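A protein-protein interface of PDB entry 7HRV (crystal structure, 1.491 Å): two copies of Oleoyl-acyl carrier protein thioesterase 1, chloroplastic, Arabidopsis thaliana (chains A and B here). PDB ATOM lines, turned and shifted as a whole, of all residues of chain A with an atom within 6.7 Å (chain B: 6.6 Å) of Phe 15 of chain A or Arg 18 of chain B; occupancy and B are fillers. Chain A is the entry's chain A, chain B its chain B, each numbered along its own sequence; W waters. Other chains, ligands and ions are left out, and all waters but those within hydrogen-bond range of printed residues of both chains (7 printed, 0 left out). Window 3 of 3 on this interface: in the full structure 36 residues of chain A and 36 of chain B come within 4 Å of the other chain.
The backbone NH of Val 87 of chain A sits at hydrogen-bond distance from the backbone carbonyl oxygen of Phe 15 of chain A (2.9 Å).
OH of Tyr 20 of chain A lies within hydrogen-bond range of NH1 of Arg 18 of chain A, at 2.9 Å.
N of Arg 18 of chain A sits at hydrogen-bond distance from OE1 of Glu 21 of chain A (2.8 Å).
The guanidinium group (NH1) of Arg 18 of chain B lies within hydrogen-bond range of the side-chain hydroxyl (OH) of Tyr 20 of chain B, at 2.9 Å.
The backbone NH (N) of Arg 18 of chain B is in hydrogen-bond range of the side-chain carboxylate (OE1) of Glu 21 of chain B (2.8 Å).
The side-chain hydroxyl (OG1) of Thr 32 of chain B is in hydrogen-bond range of the backbone carbonyl oxygen (O) of Glu 21 of chain B (2.7 Å).
Arg 18 of chain B touches its own counterpart, Arg 18 of chain A.
Arg 18 of chain A touches Glu 21 of chain B, and with the chains exchanged Glu 21 of chain A touches Arg 18 of chain B.
Tyr 20 of chain A touches Glu 21 of chain B, and with the chains exchanged Glu 21 of chain A touches Tyr 20 of chain B.
Positions printed for both chains: 16, 17, 18, 20, 21, 32, 84 and 85.
Printed residues of chain A that touch a printed residue of chain B: Phe 15, Arg 18, Tyr 20, Glu 21, Asn 35, Leu 36, Glu 39 and Met 190.
Of the 12 printed residues of chain B, 6 touch a printed residue of chain A.
Hydrophobic or aromatic side chains of chain B that line the printed part of chain A: Tyr 20, Val 22 and Trp 83.
Among the printed residues, 13 pairs touch across the chains.
Among the printed residues, Asp or Glu carboxylates within 4 Å of a Lys or Arg side-chain nitrogen of the other chain: Arg 18 of chain A with Glu 21 of chain B (2.9 Å) and Glu 21 of chain A with Arg 18 of chain B (2.9 Å).
Of chain B, only Arg 18 (3.7 Å) comes within 4 Å of Phe 15 of chain A.
Printed residues of chain A within 4 Å of Arg 18 of chain B: Phe 15, Arg 18, Glu 21, Leu 36 and Glu 39.
Printed residues of chain A within 4 Å of Glu 21 of chain B: Arg 18 and Tyr 20.
Of the printed residues of chain B, Arg 18 of chain A touches Arg 18 and Glu 21.
The nearest printed residue of chain B that does not touch Phe 15 of chain A is Tyr 20 of chain B (6.7 Å).
The nearest printed residue of chain B that does not touch Tyr 20 of chain A is Arg 18 of chain B (5.5 Å).
The guanidinium group (NH1) of Arg 18 of chain A lies within salt-bridge range of the side-chain carboxylate (OE2) of Glu 21 of chain B.
The side-chain carboxylate (OE2) of Glu 21 of chain A is in salt-bridge range of the guanidinium group (NH1) of Arg 18 of chain B, at 2.9 Å.
The side-chain carboxylate of Glu 39 of chain A sits at hydrogen-bond distance from the backbone NH of Ser 19 of chain B (2.8 Å).
The guanidinium group (NH2) of Arg 18 of chain A lies close to the guanidinium group (NH2) of Arg 18 of chain B, at 3.4 Å.
Among the printed residues, pairs that only touch across the chains: Phe 15 of chain A with Arg 18 of chain B, Tyr 20 of chain A with Glu 21 of chain B, Glu 21 of chain A with Tyr 20 of chain B, Asn 35 of chain A with Tyr 20 of chain B, Leu 36 of chain A with Arg 18 of chain B, Glu 39 of chain A with Arg 18 of chain B, Met 190 of chain A with Ser 19 of chain B, Met 190 of chain A with Val 22 of chain B and Met 190 of chain A with Trp 83 of chain B.
Water W5 bridges the side-chain carboxylate of Glu 21 of chain A (2.6 Å) and the side-chain hydroxyl of Tyr 20 of chain B (2.6 Å).
Water W6 lies within hydrogen-bond range of OE2 of Glu 21 of chain B and OH of Tyr 20 of chain A.
Water W7 lies within hydrogen-bond range of the backbone carbonyl oxygen of Val 17 of chain B (2.8 Å) and the side-chain carboxylate of Glu 39 of chain A (3.0 Å).
Water W4 lies within hydrogen-bond range of the backbone carbonyl oxygen of Val 16 of chain A (2.8 Å), the side-chain carboxylate of Glu 21 of chain A (2.8 Å) and the guanidinium group of Arg 18 of chain B (2.8 Å).
Water W2 lies within hydrogen-bond range of O of Val 16 of chain B (2.8 Å), OE1 of Glu 21 of chain B (2.8 Å) and NH2 of Arg 18 of chain A (2.8 Å).
Water W3 bridges the backbone carbonyl oxygen of Ser 19 of chain B (2.8 Å) and the backbone NH of Met 190 of chain A (3.0 Å).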
ATOM      1  N   GLU A  13      27.210 -28.800   1.618  1.00  0.00           N
ATOM      2  CA  GLU A  13      27.908 -27.618   1.130  1.00  0.00           C
ATOM      3  C   GLU A  13      29.267 -27.529   1.774  1.00  0.00           C
ATOM      4  O   GLU A  13      29.420 -27.848   2.971  1.00  0.00           O
ATOM      5  CB  GLU A  13      27.113 -26.325   1.424  1.00  0.00           C
ATOM      6  CG  GLU A  13      27.687 -25.077   0.750  1.00  0.00           C
ATOM      7  CD  GLU A  13      26.795 -23.848   0.835  1.00  0.00           C
ATOM      8  OE1 GLU A  13      25.628 -23.988   1.274  1.00  0.00           O
ATOM      9  OE2 GLU A  13      27.255 -22.749   0.431  1.00  0.00           O
ATOM     10  N   LYS A  14      30.250 -27.080   1.006  1.00  0.00           N
ATOM     11  CA  LYS A  14      31.623 -26.899   1.505  1.00  0.00           C
ATOM     12  C   LYS A  14      31.902 -25.387   1.708  1.00  0.00           C
ATOM     13  O   LYS A  14      31.459 -24.558   0.894  1.00  0.00           O
ATOM     14  CB  LYS A  14      32.651 -27.443   0.482  1.00  0.00           C
ATOM     15  CG  LYS A  14      32.628 -28.953   0.344  1.00  0.00           C
ATOM     16  CD  LYS A  14      33.695 -29.412  -0.674  1.00  0.00           C
ATOM     17  CE  LYS A  14      33.458 -30.855  -1.059  1.00  0.00           C
ATOM     18  NZ  LYS A  14      34.145 -31.203  -2.339  1.00  0.00           N
ATOM     19  N   PHE A  15      32.632 -25.039   2.775  1.00  0.00           N
ATOM     20  CA  PHE A  15      32.989 -23.659   3.091  1.00  0.00           C
ATOM     21  C   PHE A  15      34.480 -23.573   3.371  1.00  0.00           C
ATOM     22  O   PHE A  15      35.019 -24.414   4.102  1.00  0.00           O
ATOM     23  CB  PHE A  15      32.245 -23.188   4.358  1.00  0.00           C
ATOM     24  CG  PHE A  15      30.749 -23.219   4.209  1.00  0.00           C
ATOM     25  CD1 PHE A  15      30.063 -22.128   3.682  1.00  0.00           C
ATOM     26  CD2 PHE A  15      30.017 -24.296   4.671  1.00  0.00           C
ATOM     27  CE1 PHE A  15      28.667 -22.147   3.589  1.00  0.00           C
ATOM     28  CE2 PHE A  15      28.633 -24.318   4.577  1.00  0.00           C
ATOM     29  CZ  PHE A  15      27.964 -23.249   4.027  1.00  0.00           C
ATOM     30  N   VAL A  16      35.127 -22.530   2.840  1.00  0.00           N
ATOM     31  CA  VAL A  16      36.520 -22.255   3.141  1.00  0.00           C
ATOM     32  C   VAL A  16      36.520 -21.251   4.302  1.00  0.00           C
ATOM     33  O   VAL A  16      35.960 -20.164   4.159  1.00  0.00           O
ATOM     34  CB  VAL A  16      37.249 -21.671   1.891  1.00  0.00           C
ATOM     35  CG1 VAL A  16      38.668 -21.270   2.247  1.00  0.00           C
ATOM     36  CG2 VAL A  16      37.264 -22.687   0.750  1.00  0.00           C
ATOM     37  N   VAL A  17      37.112 -21.606   5.451  1.00  0.00           N
ATOM     38  CA  VAL A  17      37.139 -20.709   6.621  1.00  0.00           C
ATOM     39  C   VAL A  17      37.920 -19.395   6.346  1.00  0.00           C
ATOM     40  O   VAL A  17      39.086 -19.422   5.934  1.00  0.00           O
ATOM     41  CB  VAL A  17      37.677 -21.447   7.865  1.00  0.00           C
ATOM     42  CG1 VAL A  17      37.706 -20.526   9.082  1.00  0.00           C
ATOM     43  CG2 VAL A  17      36.835 -22.694   8.158  1.00  0.00           C
ATOM     44  N   ARG A  18      37.245 -18.246   6.557  1.00  0.00           N
ATOM     45  CA  ARG A  18      37.814 -16.921   6.280  1.00  0.00           C
ATOM     46  C   ARG A  18      38.675 -16.365   7.389  1.00  0.00           C
ATOM     47  O   ARG A  18      38.514 -16.734   8.566  1.00  0.00           O
ATOM     48  CB  ARG A  18      36.686 -15.930   5.918  1.00  0.00           C
ATOM     49  CG  ARG A  18      35.909 -16.396   4.681  1.00  0.00           C
ATOM     50  CD  ARG A  18      34.760 -15.460   4.307  1.00  0.00           C
ATOM     51  NE  ARG A  18      34.049 -15.936   3.120  1.00  0.00           N
ATOM     52  CZ  ARG A  18      32.862 -15.460   2.730  1.00  0.00           C
ATOM     53  NH1 ARG A  18      32.266 -14.487   3.420  1.00  0.00           N
ATOM     54  NH2 ARG A  18      32.268 -15.946   1.641  1.00  0.00           N
ATOM     55  N   TYR A  20      38.574 -13.448   8.888  1.00  0.00           N
ATOM     56  CA  TYR A  20      37.843 -12.745   9.964  1.00  0.00           C
ATOM     57  C   TYR A  20      36.901 -13.650  10.794  1.00  0.00           C
ATOM     58  O   TYR A  20      36.267 -13.168  11.763  1.00  0.00           O
ATOM     59  CB  TYR A  20      37.082 -11.528   9.402  1.00  0.00           C
ATOM     60  CG  TYR A  20      36.044 -11.867   8.346  1.00  0.00           C
ATOM     61  CD1 TYR A  20      34.757 -12.243   8.706  1.00  0.00           C
ATOM     62  CD2 TYR A  20      36.347 -11.788   6.984  1.00  0.00           C
ATOM     63  CE1 TYR A  20      33.790 -12.525   7.740  1.00  0.00           C
ATOM     64  CE2 TYR A  20      35.385 -12.062   6.011  1.00  0.00           C
ATOM     65  CZ  TYR A  20      34.104 -12.438   6.399  1.00  0.00           C
ATOM     66  OH  TYR A  20      33.125 -12.665   5.456  1.00  0.00           O
ATOM     67  N   GLU A  21      36.781 -14.926  10.365  1.00  0.00           N
ATOM     68  CA  GLU A  21      35.916 -15.897  11.015  1.00  0.00           C
ATOM     69  C   GLU A  21      36.594 -16.658  12.162  1.00  0.00           C
ATOM     70  O   GLU A  21      35.927 -17.458  12.815  1.00  0.00           O
ATOM     71  CB  GLU A  21      35.419 -16.910   9.945  1.00  0.00           C
ATOM     72  CG  GLU A  21      34.373 -16.318   8.997  1.00  0.00           C
ATOM     73  CD  GLU A  21      33.878 -17.273   7.908  1.00  0.00           C
ATOM     74  OE1 GLU A  21      34.599 -18.250   7.579  1.00  0.00           O
ATOM     75  OE2 GLU A  21      32.782 -17.021   7.349  1.00  0.00           O
ATOM     76  N   THR A  32      31.070 -18.453  14.119  1.00  0.00           N
ATOM     77  CA  THR A  32      31.267 -18.771  12.684  1.00  0.00           C
ATOM     78  C   THR A  32      30.586 -20.120  12.326  1.00  0.00           C
ATOM     79  O   THR A  32      29.804 -20.186  11.380  1.00  0.00           O
ATOM     80  CB  THR A  32      32.755 -18.812  12.340  1.00  0.00           C
ATOM     81  OG1 THR A  32      33.239 -17.455  12.386  1.00  0.00           O
ATOM     82  CG2 THR A  32      33.027 -19.475  10.962  1.00  0.00           C
ATOM     83  N   ASN A  35      26.868 -19.610  12.097  1.00  0.00           N
ATOM     84  CA  ASN A  35      26.495 -18.884  10.862  1.00  0.00           C
ATOM     85  C   ASN A  35      26.538 -19.867   9.653  1.00  0.00           C
ATOM     86  O   ASN A  35      25.638 -19.830   8.795  1.00  0.00           O
ATOM     87  CB  ASN A  35      27.510 -17.751  10.624  1.00  0.00           C
ATOM     88  CG  ASN A  35      27.100 -16.487  11.345  1.00  0.00           C
ATOM     89  OD1 ASN A  35      25.910 -16.175  11.411  1.00  0.00           O
ATOM     90  ND2 ASN A  35      28.066 -15.728  11.879  1.00  0.00           N
ATOM     91  N   LEU A  36      27.567 -20.732   9.597  1.00  0.00           N
ATOM     92  CA  LEU A  36      27.640 -21.705   8.462  1.00  0.00           C
ATOM     93  C   LEU A  36      26.456 -22.702   8.525  1.00  0.00           C
ATOM     94  O   LEU A  36      25.843 -23.031   7.502  1.00  0.00           O
ATOM     95  CB  LEU A  36      28.965 -22.467   8.501  1.00  0.00           C
ATOM     96  CG  LEU A  36      30.252 -21.607   8.418  1.00  0.00           C
ATOM     97  CD1 LEU A  36      31.485 -22.503   8.314  1.00  0.00           C
ATOM     98  CD2 LEU A  36      30.204 -20.637   7.223  1.00  0.00           C
ATOM     99  N   LEU A  37      26.079 -23.134   9.753  1.00  0.00           N
ATOM    100  CA  LEU A  37      24.912 -24.042   9.892  1.00  0.00           C
ATOM    101  C   LEU A  37      23.656 -23.341   9.355  1.00  0.00           C
ATOM    102  O   LEU A  37      22.863 -23.947   8.620  1.00  0.00           O
ATOM    103  CB  LEU A  37      24.670 -24.392  11.377  1.00  0.00           C
ATOM    104  CG  LEU A  37      25.794 -25.115  12.112  1.00  0.00           C
ATOM    105  CD1 LEU A  37      25.320 -25.471  13.530  1.00  0.00           C
ATOM    106  CD2 LEU A  37      26.235 -26.409  11.390  1.00  0.00           C
ATOM    107  N   GLU A  39      23.542 -20.879   7.109  1.00  0.00           N
ATOM    108  CA  GLU A  39      23.672 -20.679   5.660  1.00  0.00           C
ATOM    109  C   GLU A  39      23.336 -21.977   4.901  1.00  0.00           C
ATOM    110  O   GLU A  39      22.567 -21.936   3.923  1.00  0.00           O
ATOM    111  CB  GLU A  39      25.082 -20.195   5.309  1.00  0.00           C
ATOM    112  CG  GLU A  39      25.366 -20.148   3.800  1.00  0.00           C
ATOM    113  CD  GLU A  39      24.603 -19.136   2.957  1.00  0.00           C
ATOM    114  OE1 GLU A  39      23.741 -18.420   3.517  1.00  0.00           O
ATOM    115  OE2 GLU A  39      24.856 -19.058   1.726  1.00  0.00           O
ATOM    116  N   VAL A  40      23.887 -23.127   5.353  1.00  0.00           N
ATOM    117  CA  VAL A  40      23.573 -24.384   4.640  1.00  0.00           C
ATOM    118  C   VAL A  40      22.073 -24.742   4.818  1.00  0.00           C
ATOM    119  O   VAL A  40      21.417 -25.217   3.865  1.00  0.00           O
ATOM    120  CB  VAL A  40      24.542 -25.544   4.965  1.00  0.00           C
ATOM    121  CG1 VAL A  40      24.408 -26.023   6.415  1.00  0.00           C
ATOM    122  CG2 VAL A  40      24.363 -26.706   3.957  1.00  0.00           C
ATOM    123  N   ASN A  43      20.276 -22.669   2.210  1.00  0.00           N
ATOM    124  CA  ASN A  43      20.490 -23.180   0.838  1.00  0.00           C
ATOM    125  C   ASN A  43      19.667 -24.465   0.604  1.00  0.00           C
ATOM    126  O   ASN A  43      19.052 -24.636  -0.473  1.00  0.00           O
ATOM    127  CB  ASN A  43      21.975 -23.317   0.513  1.00  0.00           C
ATOM    128  CG  ASN A  43      22.620 -21.941   0.445  1.00  0.00           C
ATOM    129  OD1 ASN A  43      21.968 -20.926   0.077  1.00  0.00           O
ATOM    130  ND2 ASN A  43      23.886 -21.862   0.750  1.00  0.00           N
ATOM    131  N   GLY A  84      41.428 -21.057   6.353  1.00  0.00           N
ATOM    132  CA  GLY A  84      41.823 -21.611   5.067  1.00  0.00           C
ATOM    133  C   GLY A  84      41.414 -23.065   4.848  1.00  0.00           C
ATOM    134  O   GLY A  84      41.479 -23.565   3.714  1.00  0.00           O
ATOM    135  N   ASP A  85      41.029 -23.774   5.935  1.00  0.00           N
ATOM    136  CA  ASP A  85      40.565 -25.170   5.808  1.00  0.00           C
ATOM    137  C   ASP A  85      39.177 -25.212   5.143  1.00  0.00           C
ATOM    138  O   ASP A  85      38.410 -24.241   5.205  1.00  0.00           O
ATOM    139  CB  ASP A  85      40.424 -25.828   7.192  1.00  0.00           C
ATOM    140  CG  ASP A  85      41.706 -26.308   7.854  1.00  0.00           C
ATOM    141  OD1 ASP A  85      42.777 -26.190   7.228  1.00  0.00           O
ATOM    142  OD2 ASP A  85      41.625 -26.814   9.019  1.00  0.00           O
ATOM    143  N   VAL A  86      38.826 -26.368   4.566  1.00  0.00           N
ATOM    144  CA  VAL A  86      37.510 -26.547   3.949  1.00  0.00           C
ATOM    145  C   VAL A  86      36.703 -27.467   4.863  1.00  0.00           C
ATOM    146  O   VAL A  86      37.171 -28.564   5.190  1.00  0.00           O
ATOM    147  CB  VAL A  86      37.643 -27.186   2.550  1.00  0.00           C
ATOM    148  CG1 VAL A  86      36.261 -27.458   1.926  1.00  0.00           C
ATOM    149  CG2 VAL A  86      38.500 -26.306   1.634  1.00  0.00           C
ATOM    150  N   VAL A  87      35.504 -27.044   5.255  1.00  0.00           N
ATOM    151  CA  VAL A  87      34.625 -27.858   6.089  1.00  0.00           C
ATOM    152  C   VAL A  87      33.377 -28.233   5.250  1.00  0.00           C
ATOM    153  O   VAL A  87      32.868 -27.379   4.514  1.00  0.00           O
ATOM    154  CB  VAL A  87      34.237 -27.160   7.427  1.00  0.00           C
ATOM    155  CG1 VAL A  87      33.601 -25.805   7.183  1.00  0.00           C
ATOM    156  CG2 VAL A  87      33.299 -28.036   8.259  1.00  0.00           C
ATOM    157  N   GLU A  88      32.954 -29.509   5.279  1.00  0.00           N
ATOM    158  CA  GLU A  88      31.767 -29.901   4.552  1.00  0.00           C
ATOM    159  C   GLU A  88      30.662 -30.102   5.577  1.00  0.00           C
ATOM    160  O   GLU A  88      30.876 -30.773   6.587  1.00  0.00           O
ATOM    161  CB  GLU A  88      31.983 -31.204   3.747  1.00  0.00           C
ATOM    162  CG  GLU A  88      30.744 -31.534   2.909  1.00  0.00           C
ATOM    163  CD  GLU A  88      30.885 -32.744   2.002  1.00  0.00           C
ATOM    164  OE1 GLU A  88      30.979 -33.872   2.539  1.00  0.00           O
ATOM    165  OE2 GLU A  88      30.849 -32.571   0.759  1.00  0.00           O
ATOM    166  N   ILE A  89      29.497 -29.501   5.346  1.00  0.00           N
ATOM    167  CA  ILE A  89      28.384 -29.645   6.287  1.00  0.00           C
ATOM    168  C   ILE A  89      27.210 -30.287   5.548  1.00  0.00           C
ATOM    169  O   ILE A  89      26.837 -29.813   4.462  1.00  0.00           O
ATOM    170  CB  ILE A  89      27.948 -28.278   6.843  1.00  0.00           C
ATOM    171  CG1 ILE A  89      29.174 -27.524   7.413  1.00  0.00           C
ATOM    172  CG2 ILE A  89      26.851 -28.505   7.931  1.00  0.00           C
ATOM    173  CD1 ILE A  89      28.860 -26.135   8.050  1.00  0.00           C
ATOM    174  N   MET A 190      17.724 -10.206   7.242  1.00  0.00           N
ATOM    175  CA  MET A 190      17.088  -9.425   6.196  1.00  0.00           C
ATOM    176  C   MET A 190      15.649  -8.983   6.579  1.00  0.00           C
ATOM    177  O   MET A 190      15.161  -8.000   6.041  1.00  0.00           O
ATOM    178  CB  MET A 190      17.124 -10.222   4.885  1.00  0.00           C
ATOM    179  CG  MET A 190      16.305 -11.485   4.947  1.00  0.00           C
ATOM    180  SD  MET A 190      16.456 -12.398   3.376  1.00  0.00           S
ATOM    181  CE  MET A 190      17.981 -13.363   3.718  1.00  0.00           C
ATOM    182  N   VAL B  16      30.144 -16.063  -3.067  1.00  0.00           N
ATOM    183  CA  VAL B  16      28.702 -16.207  -3.197  1.00  0.00           C
ATOM    184  C   VAL B  16      28.095 -15.501  -1.979  1.00  0.00           C
ATOM    185  O   VAL B  16      28.408 -15.866  -0.845  1.00  0.00           O
ATOM    186  CB  VAL B  16      28.296 -17.713  -3.237  1.00  0.00           C
ATOM    187  CG1 VAL B  16      26.784 -17.862  -3.239  1.00  0.00           C
ATOM    188  CG2 VAL B  16      28.895 -18.409  -4.462  1.00  0.00           C
ATOM    189  N   VAL B  17      27.266 -14.478  -2.198  1.00  0.00           N
ATOM    190  CA  VAL B  17      26.669 -13.718  -1.078  1.00  0.00           C
ATOM    191  C   VAL B  17      25.740 -14.600  -0.202  1.00  0.00           C
ATOM    192  O   VAL B  17      24.804 -15.238  -0.702  1.00  0.00           O
ATOM    193  CB  VAL B  17      25.946 -12.450  -1.600  1.00  0.00           C
ATOM    194  CG1 VAL B  17      25.331 -11.654  -0.443  1.00  0.00           C
ATOM    195  CG2 VAL B  17      26.922 -11.567  -2.391  1.00  0.00           C
ATOM    196  N   ARG B  18      26.037 -14.644   1.121  1.00  0.00           N
ATOM    197  CA  ARG B  18      25.295 -15.483   2.071  1.00  0.00           C
ATOM    198  C   ARG B  18      24.020 -14.854   2.591  1.00  0.00           C
ATOM    199  O   ARG B  18      23.880 -13.611   2.612  1.00  0.00           O
ATOM    200  CB  ARG B  18      26.221 -15.873   3.245  1.00  0.00           C
ATOM    201  CG  ARG B  18      27.450 -16.665   2.746  1.00  0.00           C
ATOM    202  CD  ARG B  18      28.400 -17.061   3.869  1.00  0.00           C
ATOM    203  NE  ARG B  18      29.541 -17.814   3.354  1.00  0.00           N
ATOM    204  CZ  ARG B  18      30.648 -18.061   4.061  1.00  0.00           C
ATOM    205  NH1 ARG B  18      30.740 -17.659   5.324  1.00  0.00           N
ATOM    206  NH2 ARG B  18      31.645 -18.760   3.524  1.00  0.00           N
ATOM    207  N   SER B  19      23.104 -15.714   3.111  1.00  0.00           N
ATOM    208  CA  SER B  19      21.832 -15.275   3.664  1.00  0.00           C
ATOM    209  C   SER B  19      22.018 -14.241   4.765  1.00  0.00           C
ATOM    210  O   SER B  19      21.290 -13.247   4.804  1.00  0.00           O
ATOM    211  CB  SER B  19      21.073 -16.474   4.247  1.00  0.00           C
ATOM    212  OG  SER B  19      21.877 -17.152   5.208  1.00  0.00           O
ATOM    213  N   TYR B  20      22.972 -14.470   5.679  1.00  0.00           N
ATOM    214  CA  TYR B  20      23.133 -13.557   6.832  1.00  0.00           C
ATOM    215  C   TYR B  20      23.941 -12.278   6.528  1.00  0.00           C
ATOM    216  O   TYR B  20      24.094 -11.418   7.416  1.00  0.00           O
ATOM    217  CB  TYR B  20      23.732 -14.309   8.041  1.00  0.00           C
ATOM    218  CG  TYR B  20      25.104 -14.910   7.780  1.00  0.00           C
ATOM    219  CD1 TYR B  20      26.260 -14.154   7.943  1.00  0.00           C
ATOM    220  CD2 TYR B  20      25.244 -16.248   7.405  1.00  0.00           C
ATOM    221  CE1 TYR B  20      27.521 -14.710   7.737  1.00  0.00           C
ATOM    222  CE2 TYR B  20      26.497 -16.818   7.210  1.00  0.00           C
ATOM    223  CZ  TYR B  20      27.638 -16.041   7.380  1.00  0.00           C
ATOM    224  OH  TYR B  20      28.888 -16.587   7.232  1.00  0.00           O
ATOM    225  N   GLU B  21      24.478 -12.199   5.293  1.00  0.00           N
ATOM    226  CA  GLU B  21      25.297 -11.075   4.856  1.00  0.00           C
ATOM    227  C   GLU B  21      24.487  -9.926   4.244  1.00  0.00           C
ATOM    228  O   GLU B  21      25.082  -8.900   3.913  1.00  0.00           O
ATOM    229  CB  GLU B  21      26.323 -11.586   3.801  1.00  0.00           C
ATOM    230  CG  GLU B  21      27.455 -12.411   4.429  1.00  0.00           C
ATOM    231  CD  GLU B  21      28.474 -12.968   3.430  1.00  0.00           C
ATOM    232  OE1 GLU B  21      28.137 -13.103   2.223  1.00  0.00           O
ATOM    233  OE2 GLU B  21      29.602 -13.313   3.863  1.00  0.00           O
ATOM    234  N   VAL B  22      23.166 -10.112   4.044  1.00  0.00           N
ATOM    235  CA  VAL B  22      22.332  -9.142   3.364  1.00  0.00           C
ATOM    236  C   VAL B  22      21.446  -8.363   4.300  1.00  0.00           C
ATOM    237  O   VAL B  22      21.071  -8.864   5.365  1.00  0.00           O
ATOM    238  CB  VAL B  22      21.504  -9.786   2.203  1.00  0.00           C
ATOM    239  CG1 VAL B  22      22.415 -10.565   1.260  1.00  0.00           C
ATOM    240  CG2 VAL B  22      20.412 -10.685   2.742  1.00  0.00           C
ATOM    241  N   THR B  32      29.365  -6.249   4.879  1.00  0.00           N
ATOM    242  CA  THR B  32      29.700  -7.496   4.158  1.00  0.00           C
ATOM    243  C   THR B  32      30.752  -7.203   3.050  1.00  0.00           C
ATOM    244  O   THR B  32      31.784  -7.872   2.989  1.00  0.00           O
ATOM    245  CB  THR B  32      28.450  -8.136   3.563  1.00  0.00           C
ATOM    246  OG1 THR B  32      27.697  -8.680   4.668  1.00  0.00           O
ATOM    247  CG2 THR B  32      28.784  -9.224   2.494  1.00  0.00           C
ATOM    248  N   ALA B  82      23.092  -9.185  -4.815  1.00  0.00           N
ATOM    249  CA  ALA B  82      21.967  -9.789  -4.102  1.00  0.00           C
ATOM    250  C   ALA B  82      22.393 -11.110  -3.441  1.00  0.00           C
ATOM    251  O   ALA B  82      23.377 -11.728  -3.832  1.00  0.00           O
ATOM    252  CB  ALA B  82      20.821 -10.058  -5.085  1.00  0.00           C
ATOM    253  N   TRP B  83      21.613 -11.559  -2.455  1.00  0.00           N
ATOM    254  CA  TRP B  83      21.738 -12.863  -1.799  1.00  0.00           C
ATOM    255  C   TRP B  83      21.844 -13.992  -2.885  1.00  0.00           C
ATOM    256  O   TRP B  83      21.003 -14.025  -3.794  1.00  0.00           O
ATOM    257  CB  TRP B  83      20.437 -13.016  -0.991  1.00  0.00           C
ATOM    258  CG  TRP B  83      20.206 -14.328  -0.326  1.00  0.00           C
ATOM    259  CD1 TRP B  83      21.133 -15.278   0.002  1.00  0.00           C
ATOM    260  CD2 TRP B  83      18.956 -14.780   0.208  1.00  0.00           C
ATOM    261  NE1 TRP B  83      20.523 -16.323   0.653  1.00  0.00           N
ATOM    262  CE2 TRP B  83      19.177 -16.052   0.771  1.00  0.00           C
ATOM    263  CE3 TRP B  83      17.653 -14.260   0.201  1.00  0.00           C
ATOM    264  CZ2 TRP B  83      18.155 -16.778   1.385  1.00  0.00           C
ATOM    265  CZ3 TRP B  83      16.635 -15.001   0.778  1.00  0.00           C
ATOM    266  CH2 TRP B  83      16.894 -16.233   1.377  1.00  0.00           C
ATOM    267  N   GLY B  84      22.894 -14.813  -2.835  1.00  0.00           N
ATOM    268  CA  GLY B  84      23.063 -15.887  -3.811  1.00  0.00           C
ATOM    269  C   GLY B  84      23.840 -15.488  -5.063  1.00  0.00           C
ATOM    270  O   GLY B  84      24.263 -16.364  -5.835  1.00  0.00           O
ATOM    271  N   ASP B  85      24.012 -14.170  -5.300  1.00  0.00           N
ATOM    272  CA  ASP B  85      24.810 -13.701  -6.451  1.00  0.00           C
ATOM    273  C   ASP B  85      26.308 -13.979  -6.220  1.00  0.00           C
ATOM    274  O   ASP B  85      26.774 -14.083  -5.066  1.00  0.00           O
ATOM    275  CB  ASP B  85      24.649 -12.181  -6.645  1.00  0.00           C
ATOM    276  CG  ASP B  85      23.369 -11.704  -7.310  1.00  0.00           C
ATOM    277  OD1 ASP B  85      22.549 -12.560  -7.706  1.00  0.00           O
ATOM    278  OD2 ASP B  85      23.195 -10.450  -7.438  1.00  0.00           O
HETATM  279  O   HOH W   1      21.526 -18.803   1.615  1.00  0.00           O
HETATM  280  O   HOH W   2      30.130 -14.371   0.744  1.00  0.00           O
HETATM  281  O   HOH W   3      19.349 -12.643   6.795  1.00  0.00           O
HETATM  282  O   HOH W   4      33.551 -19.614   5.404  1.00  0.00           O
HETATM  283  O   HOH W   5      31.023 -15.237   7.978  1.00  0.00           O
HETATM  284  O   HOH W   6      30.609 -12.968   6.234  1.00  0.00           O
HETATM  285  O   HOH W   7      23.736 -17.775  -0.708  1.00  0.00           O
